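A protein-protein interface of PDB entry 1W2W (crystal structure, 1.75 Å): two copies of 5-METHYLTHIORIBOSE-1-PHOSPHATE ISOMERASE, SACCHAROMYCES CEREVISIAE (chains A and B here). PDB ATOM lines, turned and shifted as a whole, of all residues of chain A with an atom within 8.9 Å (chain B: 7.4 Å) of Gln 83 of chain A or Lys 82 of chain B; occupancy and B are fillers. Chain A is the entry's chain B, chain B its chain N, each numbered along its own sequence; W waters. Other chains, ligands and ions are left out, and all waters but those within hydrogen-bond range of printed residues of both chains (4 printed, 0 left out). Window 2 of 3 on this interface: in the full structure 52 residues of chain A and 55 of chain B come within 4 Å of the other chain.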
ATOM      1  N   ALA A  42     -19.654  15.593  -5.427  1.00  0.00           N
ATOM      2  CA  ALA A  42     -19.290  15.532  -4.010  1.00  0.00           C
ATOM      3  C   ALA A  42     -19.335  16.914  -3.361  1.00  0.00           C
ATOM      4  O   ALA A  42     -19.962  17.092  -2.313  1.00  0.00           O
ATOM      5  CB  ALA A  42     -17.916  14.863  -3.816  1.00  0.00           C
ATOM      6  N   ILE A  45     -22.925  18.179  -2.972  1.00  0.00           N
ATOM      7  CA  ILE A  45     -23.616  17.601  -1.819  1.00  0.00           C
ATOM      8  C   ILE A  45     -23.227  18.326  -0.522  1.00  0.00           C
ATOM      9  O   ILE A  45     -24.081  18.656   0.302  1.00  0.00           O
ATOM     10  CB  ILE A  45     -23.285  16.113  -1.710  1.00  0.00           C
ATOM     11  CG1 ILE A  45     -23.927  15.329  -2.860  1.00  0.00           C
ATOM     12  CG2 ILE A  45     -23.719  15.542  -0.365  1.00  0.00           C
ATOM     13  CD1 ILE A  45     -23.376  13.906  -3.006  1.00  0.00           C
ATOM     14  N   ARG A  46     -21.935  18.576  -0.349  1.00  0.00           N
ATOM     15  CA  ARG A  46     -21.448  19.178   0.887  1.00  0.00           C
ATOM     16  C   ARG A  46     -21.878  20.633   1.071  1.00  0.00           C
ATOM     17  O   ARG A  46     -21.891  21.132   2.206  1.00  0.00           O
ATOM     18  CB  ARG A  46     -19.929  19.077   0.977  1.00  0.00           C
ATOM     19  CG  ARG A  46     -19.436  17.647   1.053  1.00  0.00           C
ATOM     20  CD  ARG A  46     -18.104  17.502   1.755  1.00  0.00           C
ATOM     21  NE  ARG A  46     -18.273  17.571   3.203  1.00  0.00           N
ATOM     22  CZ  ARG A  46     -17.392  18.122   4.028  1.00  0.00           C
ATOM     23  NH1 ARG A  46     -16.278  18.656   3.548  1.00  0.00           N
ATOM     24  NH2 ARG A  46     -17.625  18.138   5.329  1.00  0.00           N
ATOM     25  N   GLN A  76     -20.162   5.755 -10.693  1.00  0.00           N
ATOM     26  CA  GLN A  76     -19.461   6.768  -9.903  1.00  0.00           C
ATOM     27  C   GLN A  76     -20.421   7.527  -9.018  1.00  0.00           C
ATOM     28  O   GLN A  76     -20.159   7.768  -7.830  1.00  0.00           O
ATOM     29  CB  GLN A  76     -18.732   7.757 -10.829  1.00  0.00           C
ATOM     30  CG  GLN A  76     -17.931   8.781 -10.062  1.00  0.00           C
ATOM     31  CD  GLN A  76     -16.707   9.197 -10.818  1.00  0.00           C
ATOM     32  OE1 GLN A  76     -15.821   8.372 -11.074  1.00  0.00           O
ATOM     33  NE2 GLN A  76     -16.649  10.469 -11.197  1.00  0.00           N
ATOM     34  N   LEU A  77     -21.552   7.908  -9.603  1.00  0.00           N
ATOM     35  CA  LEU A  77     -22.582   8.598  -8.844  1.00  0.00           C
ATOM     36  C   LEU A  77     -23.073   7.711  -7.693  1.00  0.00           C
ATOM     37  O   LEU A  77     -23.319   8.200  -6.592  1.00  0.00           O
ATOM     38  CB  LEU A  77     -23.731   8.995  -9.788  1.00  0.00           C
ATOM     39  CG  LEU A  77     -24.985   9.592  -9.131  1.00  0.00           C
ATOM     40  CD1 LEU A  77     -24.643  10.883  -8.380  1.00  0.00           C
ATOM     41  CD2 LEU A  77     -26.032   9.890 -10.205  1.00  0.00           C
ATOM     42  N   ALA A  78     -23.222   6.410  -7.934  1.00  0.00           N
ATOM     43  CA  ALA A  78     -23.750   5.517  -6.901  1.00  0.00           C
ATOM     44  C   ALA A  78     -22.745   5.436  -5.751  1.00  0.00           C
ATOM     45  O   ALA A  78     -23.122   5.408  -4.575  1.00  0.00           O
ATOM     46  CB  ALA A  78     -24.035   4.127  -7.465  1.00  0.00           C
ATOM     47  N   VAL A  79     -21.463   5.413  -6.098  1.00  0.00           N
ATOM     48  CA  VAL A  79     -20.423   5.316  -5.077  1.00  0.00           C
ATOM     49  C   VAL A  79     -20.399   6.587  -4.222  1.00  0.00           C
ATOM     50  O   VAL A  79     -20.254   6.538  -3.000  1.00  0.00           O
ATOM     51  CB  VAL A  79     -19.050   5.128  -5.724  1.00  0.00           C
ATOM     52  CG1 VAL A  79     -17.942   5.332  -4.684  1.00  0.00           C
ATOM     53  CG2 VAL A  79     -18.968   3.749  -6.370  1.00  0.00           C
ATOM     54  N   ILE A  80     -20.531   7.737  -4.875  1.00  0.00           N
ATOM     55  CA  ILE A  80     -20.584   8.995  -4.146  1.00  0.00           C
ATOM     56  C   ILE A  80     -21.826   9.060  -3.263  1.00  0.00           C
ATOM     57  O   ILE A  80     -21.743   9.462  -2.104  1.00  0.00           O
ATOM     58  CB  ILE A  80     -20.524  10.188  -5.125  1.00  0.00           C
ATOM     59  CG1 ILE A  80     -19.191  10.182  -5.865  1.00  0.00           C
ATOM     60  CG2 ILE A  80     -20.706  11.510  -4.386  1.00  0.00           C
ATOM     61  CD1 ILE A  80     -19.167  11.046  -7.115  1.00  0.00           C
ATOM     62  N   CYS A  81     -22.977   8.664  -3.797  1.00  0.00           N
ATOM     63  CA  CYS A  81     -24.184   8.568  -2.978  1.00  0.00           C
ATOM     64  C   CYS A  81     -24.011   7.671  -1.757  1.00  0.00           C
ATOM     65  O   CYS A  81     -24.503   7.989  -0.675  1.00  0.00           O
ATOM     66  CB  CYS A  81     -25.373   8.097  -3.821  1.00  0.00           C
ATOM     67  SG  CYS A  81     -25.979   9.422  -4.907  1.00  0.00           S
ATOM     68  N   LYS A  82     -23.307   6.559  -1.930  1.00  0.00           N
ATOM     69  CA  LYS A  82     -23.016   5.675  -0.803  1.00  0.00           C
ATOM     70  C   LYS A  82     -22.194   6.403   0.258  1.00  0.00           C
ATOM     71  O   LYS A  82     -22.532   6.359   1.439  1.00  0.00           O
ATOM     72  CB  LYS A  82     -22.299   4.401  -1.260  1.00  0.00           C
ATOM     73  CG  LYS A  82     -21.861   3.485  -0.115  1.00  0.00           C
ATOM     74  CD  LYS A  82     -20.993   2.314  -0.604  1.00  0.00           C
ATOM     75  CE  LYS A  82     -20.124   1.767   0.540  1.00  0.00           C
ATOM     76  NZ  LYS A  82     -19.011   0.868   0.098  1.00  0.00           N
ATOM     77  N   GLN A  83     -21.126   7.070  -0.165  1.00  0.00           N
ATOM     78  CA  GLN A  83     -20.273   7.834   0.752  1.00  0.00           C
ATOM     79  C   GLN A  83     -21.088   8.819   1.595  1.00  0.00           C
ATOM     80  O   GLN A  83     -20.858   8.971   2.799  1.00  0.00           O
ATOM     81  CB  GLN A  83     -19.200   8.598  -0.030  1.00  0.00           C
ATOM     82  CG  GLN A  83     -18.418   9.598   0.842  1.00  0.00           C
ATOM     83  CD  GLN A  83     -17.378   8.925   1.734  1.00  0.00           C
ATOM     84  OE1 GLN A  83     -17.015   7.763   1.521  1.00  0.00           O
ATOM     85  NE2 GLN A  83     -16.891   9.660   2.733  1.00  0.00           N
ATOM     86  N   PHE A  84     -22.025   9.503   0.950  1.00  0.00           N
ATOM     87  CA  PHE A  84     -22.789  10.566   1.589  1.00  0.00           C
ATOM     88  C   PHE A  84     -24.156  10.145   2.123  1.00  0.00           C
ATOM     89  O   PHE A  84     -24.925  10.984   2.588  1.00  0.00           O
ATOM     90  CB  PHE A  84     -22.900  11.781   0.658  1.00  0.00           C
ATOM     91  CG  PHE A  84     -21.600  12.500   0.478  1.00  0.00           C
ATOM     92  CD1 PHE A  84     -21.175  13.419   1.425  1.00  0.00           C
ATOM     93  CD2 PHE A  84     -20.788  12.258  -0.623  1.00  0.00           C
ATOM     94  CE1 PHE A  84     -19.972  14.081   1.279  1.00  0.00           C
ATOM     95  CE2 PHE A  84     -19.583  12.920  -0.774  1.00  0.00           C
ATOM     96  CZ  PHE A  84     -19.170  13.835   0.176  1.00  0.00           C
ATOM     97  N   GLY A  85     -24.452   8.851   2.066  1.00  0.00           N
ATOM     98  CA  GLY A  85     -25.680   8.316   2.629  1.00  0.00           C
ATOM     99  C   GLY A  85     -26.914   8.795   1.890  1.00  0.00           C
ATOM    100  O   GLY A  85     -27.981   8.957   2.496  1.00  0.00           O
ATOM    101  N   ILE A  86     -26.785   9.022   0.583  1.00  0.00           N
ATOM    102  CA  ILE A  86     -27.923   9.467  -0.223  1.00  0.00           C
ATOM    103  C   ILE A  86     -28.544   8.285  -0.970  1.00  0.00           C
ATOM    104  O   ILE A  86     -27.837   7.502  -1.591  1.00  0.00           O
ATOM    105  CB  ILE A  86     -27.477  10.566  -1.219  1.00  0.00           C
ATOM    106  CG1 ILE A  86     -27.053  11.810  -0.437  1.00  0.00           C
ATOM    107  CG2 ILE A  86     -28.602  10.883  -2.233  1.00  0.00           C
ATOM    108  CD1 ILE A  86     -26.170  12.748  -1.243  1.00  0.00           C
ATOM    109  N   LYS A  87     -29.863   8.141  -0.903  1.00  0.00           N
ATOM    110  CA  LYS A  87     -30.512   7.023  -1.583  1.00  0.00           C
ATOM    111  C   LYS A  87     -30.284   7.096  -3.090  1.00  0.00           C
ATOM    112  O   LYS A  87     -30.386   8.165  -3.683  1.00  0.00           O
ATOM    113  CB  LYS A  87     -32.012   7.022  -1.291  1.00  0.00           C
ATOM    114  CG  LYS A  87     -32.343   6.693   0.157  1.00  0.00           C
ATOM    115  CD  LYS A  87     -32.332   5.202   0.397  1.00  0.00           C
ATOM    116  CE  LYS A  87     -33.008   4.848   1.727  1.00  0.00           C
ATOM    117  NZ  LYS A  87     -32.410   5.652   2.829  1.00  0.00           N
ATOM    118  N   LEU A 166     -25.001  -1.442  -4.652  1.00  0.00           N
ATOM    119  CA  LEU A 166     -25.039   0.025  -4.563  1.00  0.00           C
ATOM    120  C   LEU A 166     -26.393   0.671  -4.884  1.00  0.00           C
ATOM    121  O   LEU A 166     -26.535   1.903  -4.815  1.00  0.00           O
ATOM    122  CB  LEU A 166     -23.988   0.609  -5.501  1.00  0.00           C
ATOM    123  CG  LEU A 166     -22.531   0.348  -5.120  1.00  0.00           C
ATOM    124  CD1 LEU A 166     -21.629   0.862  -6.236  1.00  0.00           C
ATOM    125  CD2 LEU A 166     -22.201   1.015  -3.787  1.00  0.00           C
ATOM    126  N   GLN B  76     -14.012  14.952  -4.857  1.00  0.00           N
ATOM    127  CA  GLN B  76     -14.710  13.799  -5.426  1.00  0.00           C
ATOM    128  C   GLN B  76     -13.721  12.675  -5.712  1.00  0.00           C
ATOM    129  O   GLN B  76     -13.987  11.521  -5.389  1.00  0.00           O
ATOM    130  CB  GLN B  76     -15.394  14.212  -6.733  1.00  0.00           C
ATOM    131  CG  GLN B  76     -16.179  13.075  -7.396  1.00  0.00           C
ATOM    132  CD  GLN B  76     -17.350  13.601  -8.183  1.00  0.00           C
ATOM    133  OE1 GLN B  76     -18.237  14.255  -7.625  1.00  0.00           O
ATOM    134  NE2 GLN B  76     -17.367  13.317  -9.480  1.00  0.00           N
ATOM    135  N   LEU B  77     -12.584  13.006  -6.326  1.00  0.00           N
ATOM    136  CA  LEU B  77     -11.544  12.001  -6.516  1.00  0.00           C
ATOM    137  C   LEU B  77     -11.093  11.411  -5.183  1.00  0.00           C
ATOM    138  O   LEU B  77     -10.898  10.201  -5.067  1.00  0.00           O
ATOM    139  CB  LEU B  77     -10.373  12.577  -7.318  1.00  0.00           C
ATOM    140  CG  LEU B  77      -9.131  11.717  -7.569  1.00  0.00           C
ATOM    141  CD1 LEU B  77      -9.456  10.407  -8.310  1.00  0.00           C
ATOM    142  CD2 LEU B  77      -8.111  12.557  -8.350  1.00  0.00           C
ATOM    143  N   ALA B  78     -10.926  12.253  -4.170  1.00  0.00           N
ATOM    144  CA  ALA B  78     -10.573  11.764  -2.833  1.00  0.00           C
ATOM    145  C   ALA B  78     -11.593  10.767  -2.298  1.00  0.00           C
ATOM    146  O   ALA B  78     -11.228   9.736  -1.730  1.00  0.00           O
ATOM    147  CB  ALA B  78     -10.407  12.922  -1.858  1.00  0.00           C
ATOM    148  N   VAL B  79     -12.869  11.075  -2.484  1.00  0.00           N
ATOM    149  CA  VAL B  79     -13.935  10.204  -1.992  1.00  0.00           C
ATOM    150  C   VAL B  79     -13.904   8.879  -2.729  1.00  0.00           C
ATOM    151  O   VAL B  79     -13.980   7.820  -2.120  1.00  0.00           O
ATOM    152  CB  VAL B  79     -15.323  10.851  -2.158  1.00  0.00           C
ATOM    153  CG1 VAL B  79     -16.424   9.816  -1.934  1.00  0.00           C
ATOM    154  CG2 VAL B  79     -15.467  12.007  -1.161  1.00  0.00           C
ATOM    155  N   ILE B  80     -13.783   8.941  -4.051  1.00  0.00           N
ATOM    156  CA  ILE B  80     -13.722   7.715  -4.831  1.00  0.00           C
ATOM    157  C   ILE B  80     -12.495   6.876  -4.444  1.00  0.00           C
ATOM    158  O   ILE B  80     -12.580   5.649  -4.344  1.00  0.00           O
ATOM    159  CB  ILE B  80     -13.761   8.029  -6.347  1.00  0.00           C
ATOM    160  CG1 ILE B  80     -15.141   8.584  -6.738  1.00  0.00           C
ATOM    161  CG2 ILE B  80     -13.452   6.755  -7.132  1.00  0.00           C
ATOM    162  CD1 ILE B  80     -15.139   9.481  -7.993  1.00  0.00           C
ATOM    163  N   CYS B  81     -11.359   7.531  -4.216  1.00  0.00           N
ATOM    164  CA  CYS B  81     -10.160   6.799  -3.808  1.00  0.00           C
ATOM    165  C   CYS B  81     -10.350   6.146  -2.452  1.00  0.00           C
ATOM    166  O   CYS B  81      -9.927   5.010  -2.247  1.00  0.00           O
ATOM    167  CB  CYS B  81      -8.930   7.703  -3.783  1.00  0.00           C
ATOM    168  SG  CYS B  81      -8.265   8.096  -5.427  1.00  0.00           S
ATOM    169  N   LYS B  82     -10.984   6.857  -1.524  1.00  0.00           N
ATOM    170  CA  LYS B  82     -11.298   6.253  -0.227  1.00  0.00           C
ATOM    171  C   LYS B  82     -12.132   4.982  -0.401  1.00  0.00           C
ATOM    172  O   LYS B  82     -11.820   3.919   0.146  1.00  0.00           O
ATOM    173  CB  LYS B  82     -12.049   7.233   0.682  1.00  0.00           C
ATOM    174  CG  LYS B  82     -12.448   6.598   2.014  1.00  0.00           C
ATOM    175  CD  LYS B  82     -13.239   7.549   2.893  1.00  0.00           C
ATOM    176  CE  LYS B  82     -14.072   6.786   3.926  1.00  0.00           C
ATOM    177  NZ  LYS B  82     -15.358   6.250   3.369  1.00  0.00           N
ATOM    178  N   GLN B  83     -13.202   5.103  -1.179  1.00  0.00           N
ATOM    179  CA  GLN B  83     -14.107   3.993  -1.416  1.00  0.00           C
ATOM    180  C   GLN B  83     -13.418   2.775  -2.025  1.00  0.00           C
ATOM    181  O   GLN B  83     -13.812   1.640  -1.744  1.00  0.00           O
ATOM    182  CB  GLN B  83     -15.260   4.441  -2.314  1.00  0.00           C
ATOM    183  CG  GLN B  83     -15.988   3.280  -2.984  1.00  0.00           C
ATOM    184  CD  GLN B  83     -17.201   2.768  -2.206  1.00  0.00           C
ATOM    185  OE1 GLN B  83     -17.885   1.827  -2.664  1.00  0.00           O
ATOM    186  NE2 GLN B  83     -17.479   3.380  -1.043  1.00  0.00           N
ATOM    187  N   PHE B  84     -12.415   3.008  -2.865  1.00  0.00           N
ATOM    188  CA  PHE B  84     -11.702   1.931  -3.548  1.00  0.00           C
ATOM    189  C   PHE B  84     -10.342   1.601  -2.928  1.00  0.00           C
ATOM    190  O   PHE B  84      -9.597   0.787  -3.469  1.00  0.00           O
ATOM    191  CB  PHE B  84     -11.557   2.237  -5.047  1.00  0.00           C
ATOM    192  CG  PHE B  84     -12.825   2.023  -5.821  1.00  0.00           C
ATOM    193  CD1 PHE B  84     -13.178   0.754  -6.257  1.00  0.00           C
ATOM    194  CD2 PHE B  84     -13.669   3.081  -6.097  1.00  0.00           C
ATOM    195  CE1 PHE B  84     -14.352   0.554  -6.956  1.00  0.00           C
ATOM    196  CE2 PHE B  84     -14.844   2.891  -6.795  1.00  0.00           C
ATOM    197  CZ  PHE B  84     -15.190   1.629  -7.225  1.00  0.00           C
ATOM    198  N   GLY B  85     -10.013   2.230  -1.800  1.00  0.00           N
ATOM    199  CA  GLY B  85      -8.816   1.869  -1.050  1.00  0.00           C
ATOM    200  C   GLY B  85      -7.532   2.305  -1.728  1.00  0.00           C
ATOM    201  O   GLY B  85      -6.469   1.694  -1.559  1.00  0.00           O
ATOM    202  N   ILE B  86      -7.631   3.370  -2.516  1.00  0.00           N
ATOM    203  CA  ILE B  86      -6.488   3.887  -3.249  1.00  0.00           C
ATOM    204  C   ILE B  86      -5.870   5.075  -2.522  1.00  0.00           C
ATOM    205  O   ILE B  86      -6.573   6.020  -2.177  1.00  0.00           O
ATOM    206  CB  ILE B  86      -6.921   4.297  -4.660  1.00  0.00           C
ATOM    207  CG1 ILE B  86      -7.419   3.076  -5.438  1.00  0.00           C
ATOM    208  CG2 ILE B  86      -5.780   5.004  -5.386  1.00  0.00           C
ATOM    209  CD1 ILE B  86      -7.909   3.410  -6.836  1.00  0.00           C
ATOM    210  N   LYS B  87      -4.558   5.026  -2.290  1.00  0.00           N
ATOM    211  CA  LYS B  87      -3.871   6.123  -1.598  1.00  0.00           C
ATOM    212  C   LYS B  87      -4.036   7.447  -2.323  1.00  0.00           C
ATOM    213  O   LYS B  87      -3.927   7.508  -3.555  1.00  0.00           O
ATOM    214  CB  LYS B  87      -2.378   5.809  -1.430  1.00  0.00           C
ATOM    215  CG  LYS B  87      -2.104   4.676  -0.456  1.00  0.00           C
ATOM    216  CD  LYS B  87      -2.035   5.173   0.976  1.00  0.00           C
ATOM    217  CE  LYS B  87      -1.522   4.079   1.911  1.00  0.00           C
ATOM    218  NZ  LYS B  87      -2.617   3.111   2.210  1.00  0.00           N
ATOM    219  N   PHE B  88      -4.294   8.511  -1.565  1.00  0.00           N
ATOM    220  CA  PHE B  88      -4.595   9.814  -2.158  1.00  0.00           C
ATOM    221  C   PHE B  88      -3.618  10.831  -1.579  1.00  0.00           C
ATOM    222  O   PHE B  88      -3.588  11.023  -0.370  1.00  0.00           O
ATOM    223  CB  PHE B  88      -6.034  10.211  -1.815  1.00  0.00           C
ATOM    224  CG  PHE B  88      -6.458  11.550  -2.371  1.00  0.00           C
ATOM    225  CD1 PHE B  88      -7.077  11.637  -3.612  1.00  0.00           C
ATOM    226  CD2 PHE B  88      -6.246  12.723  -1.647  1.00  0.00           C
ATOM    227  CE1 PHE B  88      -7.475  12.869  -4.129  1.00  0.00           C
ATOM    228  CE2 PHE B  88      -6.634  13.952  -2.146  1.00  0.00           C
ATOM    229  CZ  PHE B  88      -7.247  14.032  -3.394  1.00  0.00           C
ATOM    230  N   GLU B 165      -9.126  14.385   6.594  1.00  0.00           N
ATOM    231  CA  GLU B 165      -9.405  12.975   6.851  1.00  0.00           C
ATOM    232  C   GLU B 165      -9.251  12.133   5.588  1.00  0.00           C
ATOM    233  O   GLU B 165      -8.936  10.951   5.667  1.00  0.00           O
ATOM    234  CB  GLU B 165     -10.799  12.780   7.450  1.00  0.00           C
ATOM    235  CG  GLU B 165     -11.911  13.396   6.613  1.00  0.00           C
ATOM    236  CD  GLU B 165     -13.180  12.558   6.560  1.00  0.00           C
ATOM    237  OE1 GLU B 165     -13.433  11.804   7.527  1.00  0.00           O
ATOM    238  OE2 GLU B 165     -13.929  12.659   5.553  1.00  0.00           O
ATOM    239  N   LEU B 166      -9.466  12.743   4.427  1.00  0.00           N
ATOM    240  CA  LEU B 166      -9.428  12.003   3.172  1.00  0.00           C
ATOM    241  C   LEU B 166      -8.046  12.017   2.522  1.00  0.00           C
ATOM    242  O   LEU B 166      -7.843  11.382   1.492  1.00  0.00           O
ATOM    243  CB  LEU B 166     -10.452  12.574   2.195  1.00  0.00           C
ATOM    244  CG  LEU B 166     -11.915  12.338   2.560  1.00  0.00           C
ATOM    245  CD1 LEU B 166     -12.748  12.989   1.458  1.00  0.00           C
ATOM    246  CD2 LEU B 166     -12.151  10.843   2.623  1.00  0.00           C
ATOM    247  N   ASP B 168      -4.124  11.102   2.436  1.00  0.00           N
ATOM    248  CA  ASP B 168      -3.218  10.135   3.044  1.00  0.00           C
ATOM    249  C   ASP B 168      -1.857  10.732   3.345  1.00  0.00           C
ATOM    250  O   ASP B 168      -1.164  10.264   4.248  1.00  0.00           O
ATOM    251  CB  ASP B 168      -3.081   8.902   2.161  1.00  0.00           C
ATOM    252  CG  ASP B 168      -4.370   8.119   2.097  1.00  0.00           C
ATOM    253  OD1 ASP B 168      -4.821   7.665   3.180  1.00  0.00           O
ATOM    254  OD2 ASP B 168      -4.984   7.918   1.029  1.00  0.00           O
HETATM  255  O   HOH W   1     -18.928  11.976 -12.037  1.00  0.00           O
HETATM  256  O   HOH W   2     -15.624   0.764   0.068  1.00  0.00           O
HETATM  257  O   HOH W   3     -17.416   5.404   0.292  1.00  0.00           O
HETATM  258  O   HOH W   4     -15.081  13.366 -11.043  1.00  0.00           O
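The backbone NH of Ala 42 of chain A lies within hydrogen-bond range of the side-chain amide oxygen of Gln 76 of chain B (2.9 Å).
NE2 of Gln 76 of chain A sits close to NE2 of Gln 76 of chain B.
The side-chain amide oxygen (OE1) of Gln 83 of chain B sits at hydrogen-bond distance from the side-chain amino group (NZ) of Lys 82 of chain A (3.1 Å).
The side-chain amide oxygen (OE1) of Gln 83 of chain A sits at hydrogen-bond distance from the side-chain amino group (NZ) of Lys 82 of chain B (2.9 Å).
Gln 76 of chain A touches Ile 80 of chain B (CD to CD1, 3.2 Å).
Gln 83 of chain B touches Val 79 of chain A.
CD1 of Ile 80 of chain A touches CD of Gln 76 of chain B, at 3.3 Å.
CG1 of Val 79 of chain B touches CG of Gln 83 of chain A, 3.4 Å away.
Printed residues of chain B within 4 Å of Gln 76 of chain A: Gln 76 (3.4 Å) and Ile 80 (3.2 Å).
Of the printed residues of chain B, Val 79 of chain A touches Gln 83 (3.3 Å).
Printed residues of chain B within 4 Å of Ile 80 of chain A: Gln 76 (3.3 Å).
Of chain B, only Val 79 and Lys 82 come within 4 Å of Gln 83 of chain A.
Printed residues of chain A within 4 Å of Ile 80 of chain B: Gln 76.
Of chain A, only Gln 83 (2.9 Å) comes within 4 Å of Lys 82 of chain B.
Of the printed residues of chain A, Gln 83 of chain B touches Val 79 and Lys 82.
The nearest residue of chain B that does not touch Gln 83 of chain A is Leu 166 of chain B (4.9 Å).
Hydrophobic or aromatic side chains of chain A within 4 Å of the printed part of chain B: Ala 42, Val 79 and Ile 80.
Of the 16 printed residues of chain B, 5 touch a printed residue of chain A.
Hydrophobic or aromatic side chains of chain B that line the printed part of chain A: Val 79 and Ile 80.
Among the printed residues, 8 pairs touch across the chains.
Among the printed residues, no Asp or Glu carboxylate lies within 4 Å of a Lys or Arg side-chain nitrogen of the other chain.
Gln 76 of chain B touches its own counterpart, Gln 76 of chain A.
Gln 76 of chain A touches Ile 80 of chain B, and with the chains exchanged Ile 80 of chain A touches Gln 76 of chain B.
Val 79 of chain A touches Gln 83 of chain B, and with the chains exchanged Gln 83 of chain A touches Val 79 of chain B.
Lys 82 of chain A touches Gln 83 of chain B, and with the chains exchanged Gln 83 of chain A touches Lys 82 of chain B.
Of the 8 pairs that touch across the chains among the printed residues, 7 have their exchanged pair printed and touching as well.
Water W3 lies within hydrogen-bond range of NE2 of Gln 83 of chain B and OE1 of Gln 83 of chain A.
Water W2 bridges the backbone carbonyl oxygen (O) of Gln 83 of chain B and the side-chain amino group (NZ) of Lys 82 of chain A.
Water W4 lies within hydrogen-bond range of NE2 of Gln 76 of chain B and NE2 of Gln 76 of chain A.
Water W1 bridges NE2 of Gln 76 of chain A and NE2 of Gln 76 of chain B.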
